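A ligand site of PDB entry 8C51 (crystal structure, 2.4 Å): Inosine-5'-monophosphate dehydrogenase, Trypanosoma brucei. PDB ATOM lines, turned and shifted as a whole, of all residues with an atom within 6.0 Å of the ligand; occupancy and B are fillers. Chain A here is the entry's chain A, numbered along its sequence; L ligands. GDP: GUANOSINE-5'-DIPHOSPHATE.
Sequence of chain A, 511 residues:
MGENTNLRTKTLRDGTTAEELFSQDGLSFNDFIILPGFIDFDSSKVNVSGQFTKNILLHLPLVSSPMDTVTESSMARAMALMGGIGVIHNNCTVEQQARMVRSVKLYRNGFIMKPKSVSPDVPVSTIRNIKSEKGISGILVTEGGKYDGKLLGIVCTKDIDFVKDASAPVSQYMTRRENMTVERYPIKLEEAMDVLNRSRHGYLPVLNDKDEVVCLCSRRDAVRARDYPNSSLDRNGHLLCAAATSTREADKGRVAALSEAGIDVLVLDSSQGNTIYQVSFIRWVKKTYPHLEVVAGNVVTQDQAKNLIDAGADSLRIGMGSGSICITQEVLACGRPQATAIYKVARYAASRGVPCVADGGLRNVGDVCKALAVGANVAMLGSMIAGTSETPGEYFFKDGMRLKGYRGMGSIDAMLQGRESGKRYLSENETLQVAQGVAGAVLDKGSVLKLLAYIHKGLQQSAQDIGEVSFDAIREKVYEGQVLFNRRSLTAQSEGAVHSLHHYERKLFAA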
ATOM      1  N   ARG A  99     -28.384 -40.556  -2.390  1.00  0.00           N
ATOM      2  CA  ARG A  99     -28.427 -39.489  -1.391  1.00  0.00           C
ATOM      3  C   ARG A  99     -27.018 -39.045  -0.998  1.00  0.00           C
ATOM      4  O   ARG A  99     -26.757 -37.848  -0.850  1.00  0.00           O
ATOM      5  CB  ARG A  99     -29.204 -39.952  -0.155  1.00  0.00           C
ATOM      6  CG  ARG A  99     -29.275 -38.896   0.951  1.00  0.00           C
ATOM      7  CD  ARG A  99     -30.391 -39.156   1.964  1.00  0.00           C
ATOM      8  NE  ARG A  99     -31.652 -39.530   1.332  1.00  0.00           N
ATOM      9  CZ  ARG A  99     -32.666 -38.702   1.127  1.00  0.00           C
ATOM     10  NH1 ARG A  99     -32.621 -37.429   1.490  1.00  0.00           N
ATOM     11  NH2 ARG A  99     -33.766 -39.169   0.537  1.00  0.00           N
ATOM     12  N   ARG A 102     -25.679 -36.975  -3.823  1.00  0.00           N
ATOM     13  CA  ARG A 102     -26.273 -35.643  -3.784  1.00  0.00           C
ATOM     14  C   ARG A 102     -25.628 -34.796  -2.693  1.00  0.00           C
ATOM     15  O   ARG A 102     -25.343 -33.612  -2.893  1.00  0.00           O
ATOM     16  CB  ARG A 102     -27.779 -35.751  -3.544  1.00  0.00           C
ATOM     17  CG  ARG A 102     -28.631 -35.356  -4.746  1.00  0.00           C
ATOM     18  CD  ARG A 102     -30.108 -35.531  -4.444  1.00  0.00           C
ATOM     19  NE  ARG A 102     -30.491 -36.932  -4.364  1.00  0.00           N
ATOM     20  CZ  ARG A 102     -31.024 -37.525  -3.301  1.00  0.00           C
ATOM     21  NH1 ARG A 102     -31.273 -36.852  -2.189  1.00  0.00           N
ATOM     22  NH2 ARG A 102     -31.316 -38.817  -3.363  1.00  0.00           N
ATOM     23  N   LEU A 106     -24.060 -31.233  -3.973  1.00  0.00           N
ATOM     24  CA  LEU A 106     -24.720 -29.975  -3.628  1.00  0.00           C
ATOM     25  C   LEU A 106     -24.099 -29.287  -2.427  1.00  0.00           C
ATOM     26  O   LEU A 106     -24.593 -28.229  -2.015  1.00  0.00           O
ATOM     27  CB  LEU A 106     -26.208 -30.218  -3.370  1.00  0.00           C
ATOM     28  CG  LEU A 106     -26.904 -31.077  -4.434  1.00  0.00           C
ATOM     29  CD1 LEU A 106     -28.351 -31.318  -4.079  1.00  0.00           C
ATOM     30  CD2 LEU A 106     -26.780 -30.426  -5.812  1.00  0.00           C
ATOM     31  N   TYR A 107     -23.028 -29.840  -1.875  1.00  0.00           N
ATOM     32  CA  TYR A 107     -22.303 -29.164  -0.798  1.00  0.00           C
ATOM     33  C   TYR A 107     -21.736 -27.834  -1.280  1.00  0.00           C
ATOM     34  O   TYR A 107     -21.896 -26.800  -0.630  1.00  0.00           O
ATOM     35  CB  TYR A 107     -21.198 -30.075  -0.281  1.00  0.00           C
ATOM     36  CG  TYR A 107     -20.301 -29.455   0.756  1.00  0.00           C
ATOM     37  CD1 TYR A 107     -20.772 -29.212   2.040  1.00  0.00           C
ATOM     38  CD2 TYR A 107     -18.986 -29.136   0.464  1.00  0.00           C
ATOM     39  CE1 TYR A 107     -19.959 -28.641   3.000  1.00  0.00           C
ATOM     40  CE2 TYR A 107     -18.162 -28.570   1.417  1.00  0.00           C
ATOM     41  CZ  TYR A 107     -18.651 -28.327   2.684  1.00  0.00           C
ATOM     42  OH  TYR A 107     -17.840 -27.766   3.633  1.00  0.00           O
ATOM     43  N   ASN A 109     -21.539 -24.978  -4.380  1.00  0.00           N
ATOM     44  CA  ASN A 109     -22.259 -24.452  -5.524  1.00  0.00           C
ATOM     45  C   ASN A 109     -21.749 -23.060  -5.837  1.00  0.00           C
ATOM     46  O   ASN A 109     -21.039 -22.430  -5.046  1.00  0.00           O
ATOM     47  CB  ASN A 109     -23.783 -24.386  -5.272  1.00  0.00           C
ATOM     48  CG  ASN A 109     -24.296 -25.539  -4.453  1.00  0.00           C
ATOM     49  OD1 ASN A 109     -23.892 -25.723  -3.299  1.00  0.00           O
ATOM     50  ND2 ASN A 109     -25.201 -26.315  -5.018  1.00  0.00           N
ATOM     51  N   ILE A 112     -27.010 -21.610  -5.898  1.00  0.00           N
ATOM     52  CA  ILE A 112     -27.620 -22.771  -5.265  1.00  0.00           C
ATOM     53  C   ILE A 112     -29.017 -22.973  -5.848  1.00  0.00           C
ATOM     54  O   ILE A 112     -29.924 -22.185  -5.610  1.00  0.00           O
ATOM     55  CB  ILE A 112     -27.687 -22.618  -3.740  1.00  0.00           C
ATOM     56  CG1 ILE A 112     -26.271 -22.582  -3.158  1.00  0.00           C
ATOM     57  CG2 ILE A 112     -28.528 -23.733  -3.116  1.00  0.00           C
ATOM     58  CD1 ILE A 112     -26.211 -22.690  -1.651  1.00  0.00           C
ATOM     59  N   MET A 113     -29.187 -24.043  -6.630  1.00  0.00           N
ATOM     60  CA  MET A 113     -30.477 -24.376  -7.208  1.00  0.00           C
ATOM     61  C   MET A 113     -31.254 -25.192  -6.184  1.00  0.00           C
ATOM     62  O   MET A 113     -30.675 -25.880  -5.342  1.00  0.00           O
ATOM     63  CB  MET A 113     -30.313 -25.172  -8.512  1.00  0.00           C
ATOM     64  CG  MET A 113     -29.836 -24.376  -9.732  1.00  0.00           C
ATOM     65  SD  MET A 113     -30.329 -22.641  -9.827  1.00  0.00           S
ATOM     66  CE  MET A 113     -28.825 -21.882 -10.428  1.00  0.00           C
ATOM     67  N   LYS A 114     -32.578 -25.134  -6.279  1.00  0.00           N
ATOM     68  CA  LYS A 114     -33.459 -25.822  -5.343  1.00  0.00           C
ATOM     69  C   LYS A 114     -33.022 -25.544  -3.906  1.00  0.00           C
ATOM     70  O   LYS A 114     -32.758 -26.496  -3.134  1.00  0.00           O
ATOM     71  CB  LYS A 114     -33.484 -27.317  -5.621  1.00  0.00           C
ATOM     72  CG  LYS A 114     -34.293 -27.745  -6.834  1.00  0.00           C
ATOM     73  CD  LYS A 114     -34.860 -29.139  -6.643  1.00  0.00           C
ATOM     74  CE  LYS A 114     -35.021 -29.889  -7.954  1.00  0.00           C
ATOM     75  NZ  LYS A 114     -35.991 -31.023  -7.840  1.00  0.00           N
ATOM     76  N   PRO A 115     -32.929 -24.279  -3.486  1.00  0.00           N
ATOM     77  CA  PRO A 115     -32.464 -23.994  -2.125  1.00  0.00           C
ATOM     78  C   PRO A 115     -33.440 -24.537  -1.095  1.00  0.00           C
ATOM     79  O   PRO A 115     -34.666 -24.408  -1.234  1.00  0.00           O
ATOM     80  CB  PRO A 115     -32.390 -22.459  -2.083  1.00  0.00           C
ATOM     81  CG  PRO A 115     -32.600 -21.991  -3.487  1.00  0.00           C
ATOM     82  CD  PRO A 115     -33.356 -23.057  -4.189  1.00  0.00           C
ATOM     83  N   LYS A 116     -32.902 -25.162  -0.057  1.00  0.00           N
ATOM     84  CA  LYS A 116     -33.736 -25.668   1.026  1.00  0.00           C
ATOM     85  C   LYS A 116     -34.580 -24.543   1.621  1.00  0.00           C
ATOM     86  O   LYS A 116     -34.036 -23.564   2.144  1.00  0.00           O
ATOM     87  CB  LYS A 116     -32.863 -26.295   2.115  1.00  0.00           C
ATOM     88  CG  LYS A 116     -33.639 -26.998   3.210  1.00  0.00           C
ATOM     89  CD  LYS A 116     -33.762 -28.479   2.932  1.00  0.00           C
ATOM     90  CE  LYS A 116     -35.044 -29.051   3.513  1.00  0.00           C
ATOM     91  NZ  LYS A 116     -34.980 -30.530   3.648  1.00  0.00           N
ATOM     92  N   SER A 117     -35.899 -24.690   1.542  1.00  0.00           N
ATOM     93  CA  SER A 117     -36.814 -23.691   2.076  1.00  0.00           C
ATOM     94  C   SER A 117     -37.984 -24.365   2.766  1.00  0.00           C
ATOM     95  O   SER A 117     -38.306 -25.531   2.525  1.00  0.00           O
ATOM     96  CB  SER A 117     -37.315 -22.722   1.011  1.00  0.00           C
ATOM     97  OG  SER A 117     -37.622 -23.407  -0.178  1.00  0.00           O
ATOM     98  N   LYS A 134     -28.053 -32.158   8.119  1.00  0.00           N
ATOM     99  CA  LYS A 134     -27.510 -31.861   6.794  1.00  0.00           C
ATOM    100  C   LYS A 134     -26.478 -30.738   6.794  1.00  0.00           C
ATOM    101  O   LYS A 134     -25.693 -30.650   5.841  1.00  0.00           O
ATOM    102  CB  LYS A 134     -28.641 -31.517   5.831  1.00  0.00           C
ATOM    103  CG  LYS A 134     -29.488 -32.728   5.471  1.00  0.00           C
ATOM    104  CD  LYS A 134     -30.693 -32.355   4.642  1.00  0.00           C
ATOM    105  CE  LYS A 134     -30.902 -33.339   3.500  1.00  0.00           C
ATOM    106  NZ  LYS A 134     -31.685 -32.722   2.408  1.00  0.00           N
ATOM    107  N   ILE A 136     -26.716 -27.304   6.698  1.00  0.00           N
ATOM    108  CA  ILE A 136     -26.934 -26.093   5.914  1.00  0.00           C
ATOM    109  C   ILE A 136     -27.735 -25.097   6.745  1.00  0.00           C
ATOM    110  O   ILE A 136     -28.685 -25.463   7.433  1.00  0.00           O
ATOM    111  CB  ILE A 136     -27.671 -26.385   4.584  1.00  0.00           C
ATOM    112  CG1 ILE A 136     -29.038 -26.999   4.846  1.00  0.00           C
ATOM    113  CG2 ILE A 136     -26.823 -27.297   3.703  1.00  0.00           C
ATOM    114  CD1 ILE A 136     -29.669 -27.634   3.619  1.00  0.00           C
ATOM    115  N   SER A 137     -27.339 -23.826   6.671  1.00  0.00           N
ATOM    116  CA  SER A 137     -28.032 -22.723   7.302  1.00  0.00           C
ATOM    117  C   SER A 137     -28.684 -21.847   6.224  1.00  0.00           C
ATOM    118  O   SER A 137     -28.764 -22.242   5.057  1.00  0.00           O
ATOM    119  CB  SER A 137     -27.056 -21.918   8.171  1.00  0.00           C
ATOM    120  OG  SER A 137     -27.747 -21.060   9.060  1.00  0.00           O
ATOM    121  N   GLY A 138     -29.152 -20.678   6.630  1.00  0.00           N
ATOM    122  CA  GLY A 138     -29.771 -19.768   5.687  1.00  0.00           C
ATOM    123  C   GLY A 138     -30.970 -20.376   4.996  1.00  0.00           C
ATOM    124  O   GLY A 138     -31.059 -20.356   3.765  1.00  0.00           O
ATOM    125  N   ILE A 139     -31.891 -20.924   5.771  1.00  0.00           N
ATOM    126  CA  ILE A 139     -33.066 -21.583   5.214  1.00  0.00           C
ATOM    127  C   ILE A 139     -34.049 -20.514   4.752  1.00  0.00           C
ATOM    128  O   ILE A 139     -34.389 -19.598   5.517  1.00  0.00           O
ATOM    129  CB  ILE A 139     -33.716 -22.507   6.248  1.00  0.00           C
ATOM    130  CG1 ILE A 139     -32.676 -23.378   6.964  1.00  0.00           C
ATOM    131  CG2 ILE A 139     -34.765 -23.392   5.589  1.00  0.00           C
ATOM    132  CD1 ILE A 139     -31.498 -23.849   6.103  1.00  0.00           C
ATOM    133  N   LEU A 140     -34.497 -20.622   3.518  1.00  0.00           N
ATOM    134  CA  LEU A 140     -35.459 -19.667   2.991  1.00  0.00           C
ATOM    135  C   LEU A 140     -36.865 -20.049   3.425  1.00  0.00           C
ATOM    136  O   LEU A 140     -37.205 -21.236   3.503  1.00  0.00           O
ATOM    137  CB  LEU A 140     -35.374 -19.604   1.467  1.00  0.00           C
ATOM    138  CG  LEU A 140     -33.993 -19.364   0.841  1.00  0.00           C
ATOM    139  CD1 LEU A 140     -34.124 -19.067  -0.650  1.00  0.00           C
ATOM    140  CD2 LEU A 140     -33.277 -18.235   1.549  1.00  0.00           C
ATOM    141  N   TYR A 203     -26.007 -14.831   3.012  1.00  0.00           N
ATOM    142  CA  TYR A 203     -26.790 -15.399   1.926  1.00  0.00           C
ATOM    143  C   TYR A 203     -27.403 -14.282   1.084  1.00  0.00           C
ATOM    144  O   TYR A 203     -27.639 -13.179   1.574  1.00  0.00           O
ATOM    145  CB  TYR A 203     -27.882 -16.327   2.468  1.00  0.00           C
ATOM    146  CG  TYR A 203     -27.337 -17.531   3.196  1.00  0.00           C
ATOM    147  CD1 TYR A 203     -26.868 -17.431   4.500  1.00  0.00           C
ATOM    148  CD2 TYR A 203     -27.282 -18.774   2.570  1.00  0.00           C
ATOM    149  CE1 TYR A 203     -26.359 -18.520   5.162  1.00  0.00           C
ATOM    150  CE2 TYR A 203     -26.778 -19.873   3.231  1.00  0.00           C
ATOM    151  CZ  TYR A 203     -26.314 -19.746   4.522  1.00  0.00           C
ATOM    152  OH  TYR A 203     -25.810 -20.844   5.183  1.00  0.00           O
ATOM    153  N   LEU A 216     -29.967 -19.021  -5.107  1.00  0.00           N
ATOM    154  CA  LEU A 216     -29.407 -18.546  -3.845  1.00  0.00           C
ATOM    155  C   LEU A 216     -27.886 -18.604  -3.889  1.00  0.00           C
ATOM    156  O   LEU A 216     -27.323 -19.613  -4.332  1.00  0.00           O
ATOM    157  CB  LEU A 216     -29.937 -19.388  -2.682  1.00  0.00           C
ATOM    158  CG  LEU A 216     -29.282 -19.206  -1.312  1.00  0.00           C
ATOM    159  CD1 LEU A 216     -29.571 -17.830  -0.762  1.00  0.00           C
ATOM    160  CD2 LEU A 216     -29.765 -20.280  -0.349  1.00  0.00           C
ATOM    161  N   SER A 218     -24.391 -18.303  -1.490  1.00  0.00           N
ATOM    162  CA  SER A 218     -23.957 -18.518  -0.117  1.00  0.00           C
ATOM    163  C   SER A 218     -22.523 -18.034   0.042  1.00  0.00           C
ATOM    164  O   SER A 218     -21.641 -18.430  -0.724  1.00  0.00           O
ATOM    165  CB  SER A 218     -24.073 -19.986   0.267  1.00  0.00           C
ATOM    166  OG  SER A 218     -23.002 -20.386   1.108  1.00  0.00           O
ATOM    167  N   ARG A 220     -20.692 -18.990   2.291  1.00  0.00           N
ATOM    168  CA  ARG A 220     -19.942 -20.190   2.642  1.00  0.00           C
ATOM    169  C   ARG A 220     -19.261 -20.777   1.421  1.00  0.00           C
ATOM    170  O   ARG A 220     -18.161 -21.321   1.530  1.00  0.00           O
ATOM    171  CB  ARG A 220     -20.874 -21.219   3.288  1.00  0.00           C
ATOM    172  CG  ARG A 220     -20.845 -21.202   4.804  1.00  0.00           C
ATOM    173  CD  ARG A 220     -22.212 -21.514   5.416  1.00  0.00           C
ATOM    174  NE  ARG A 220     -22.219 -21.256   6.852  1.00  0.00           N
ATOM    175  NH1 ARG A 220     -24.169 -19.994   6.873  1.00  0.00           N
ATOM    176  NH2 ARG A 220     -23.021 -20.380   8.815  1.00  0.00           N
ATOM    177  N   ARG A 224     -15.331 -21.415   1.106  1.00  0.00           N
ATOM    178  CA  ARG A 224     -14.842 -22.744   0.742  1.00  0.00           C
ATOM    179  C   ARG A 224     -13.875 -22.648  -0.438  1.00  0.00           C
ATOM    180  O   ARG A 224     -12.828 -23.297  -0.447  1.00  0.00           O
ATOM    181  CB  ARG A 224     -16.011 -23.654   0.381  1.00  0.00           C
ATOM    182  CG  ARG A 224     -16.888 -24.105   1.544  1.00  0.00           C
ATOM    183  CD  ARG A 224     -18.009 -25.009   1.040  1.00  0.00           C
ATOM    184  NE  ARG A 224     -19.345 -24.613   1.500  1.00  0.00           N
ATOM    185  CZ  ARG A 224     -19.841 -24.895   2.703  1.00  0.00           C
ATOM    186  NH1 ARG A 224     -19.114 -25.528   3.611  1.00  0.00           N
ATOM    187  NH2 ARG A 224     -21.083 -24.543   2.983  1.00  0.00           N
HETATM  188  PB  GDP L   1     -33.600 -34.470   0.475  1.00  0.00           P
HETATM  189  O1B GDP L   1     -34.431 -34.728  -0.759  1.00  0.00           O
HETATM  190  O2B GDP L   1     -34.148 -35.267   1.622  1.00  0.00           O
HETATM  191  O3B GDP L   1     -32.156 -34.889   0.228  1.00  0.00           O
HETATM  192  O3A GDP L   1     -33.640 -32.834   0.856  1.00  0.00           O
HETATM  193  PA  GDP L   1     -32.896 -31.653  -0.091  1.00  0.00           P
HETATM  194  O1A GDP L   1     -31.889 -32.325  -1.002  1.00  0.00           O
HETATM  195  O2A GDP L   1     -33.953 -30.940  -0.903  1.00  0.00           O
HETATM  196  O5' GDP L   1     -32.123 -30.564   0.887  1.00  0.00           O
HETATM  197  C5' GDP L   1     -30.884 -30.027   0.493  1.00  0.00           C
HETATM  198  C4' GDP L   1     -31.140 -28.960  -0.520  1.00  0.00           C
HETATM  199  O4' GDP L   1     -30.490 -27.511   0.036  1.00  0.00           O
HETATM  200  C3' GDP L   1     -30.602 -29.205  -1.689  1.00  0.00           C
HETATM  201  O3' GDP L   1     -31.588 -28.887  -2.742  1.00  0.00           O
HETATM  202  C2' GDP L   1     -29.376 -28.239  -1.814  1.00  0.00           C
HETATM  203  O2' GDP L   1     -29.210 -27.858  -3.069  1.00  0.00           O
HETATM  204  C1' GDP L   1     -29.803 -26.993  -0.936  1.00  0.00           C
HETATM  205  N9  GDP L   1     -28.679 -26.266  -0.365  1.00  0.00           N
HETATM  206  C8  GDP L   1     -27.381 -26.468  -0.537  1.00  0.00           C
HETATM  207  N7  GDP L   1     -26.707 -25.576   0.174  1.00  0.00           N
HETATM  208  C5  GDP L   1     -27.565 -24.785   0.814  1.00  0.00           C
HETATM  209  C6  GDP L   1     -27.429 -23.608   1.762  1.00  0.00           C
HETATM  210  O6  GDP L   1     -26.357 -23.213   2.062  1.00  0.00           O
HETATM  211  N1  GDP L   1     -28.598 -22.965   2.288  1.00  0.00           N
HETATM  212  C2  GDP L   1     -29.906 -23.437   1.905  1.00  0.00           C
HETATM  213  N2  GDP L   1     -31.110 -22.821   2.422  1.00  0.00           N
HETATM  214  N3  GDP L   1     -30.038 -24.577   1.000  1.00  0.00           N
HETATM  215  C4  GDP L   1     -28.824 -25.229   0.467  1.00  0.00           C
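NZ of Lys 134 is in salt-bridge range of O3B of the ligand (3.1 Å).
NH1 of Arg 99 lies within salt-bridge range of O2B of the ligand (2.7 Å).
The backbone carbonyl oxygen of Lys 114 sits at hydrogen-bond distance from an oxygen (O3') of the ligand.
O of Gly 138 is in hydrogen-bond range of N2 of the ligand (2.8 Å).
O of Ser 137 lies within hydrogen-bond range of N1 of the ligand, 2.9 Å away.
A nitrogen (N3) of the ligand is in hydrogen-bond range of the backbone NH (N) of Lys 116, at 3.1 Å.
The backbone carbonyl oxygen (O) of Lys 116 lies within hydrogen-bond range of a nitrogen (N2) of the ligand (3.0 Å).
An oxygen (O3B) of the ligand is in salt-bridge range of the guanidinium group (NH1) of Arg 102.
O2' of the ligand lies within hydrogen-bond range of O of Met 113 (3.4 Å).
Merely in contact with the ligand: Leu 106 (3.6 Å), Ile 112 (3.5 Å), Pro 115 (3.996 Å), Ile 136 (3.7 Å), Ile 139 (3.6 Å), Tyr 203 (3.6 Å) and Leu 216 (3.9 Å).
Within 4 Å of the ligand: Arg 99, Arg 102, Leu 106, Ile 112, Met 113, Lys 114, Pro 115, Lys 116, Lys 134, Ile 136, Ser 137, Gly 138, Ile 139, Tyr 203 and Leu 216.
The backbone carbonyl oxygen (O) of Ser 137 lies close to the side-chain hydroxyl (OH) of Tyr 203 (3.3 Å).
O of Lys 116 lies within hydrogen-bond range of N of Leu 140, at 3.3 Å.
The backbone NH (N) of Ile 112 sits at hydrogen-bond distance from the backbone carbonyl oxygen (O) of Leu 216.
The guanidinium group (NH1) of Arg 220 sits at hydrogen-bond distance from the side-chain hydroxyl (OH) of Tyr 203, 2.5 Å away.
The backbone carbonyl oxygen (O) of Leu 106 sits close to the side-chain amide oxygen (OD1) of Asn 109 (2.9 Å).
The backbone carbonyl oxygen (O) of Pro 115 is in hydrogen-bond range of the side-chain hydroxyl (OG) of Ser 117, at 3.3 Å.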
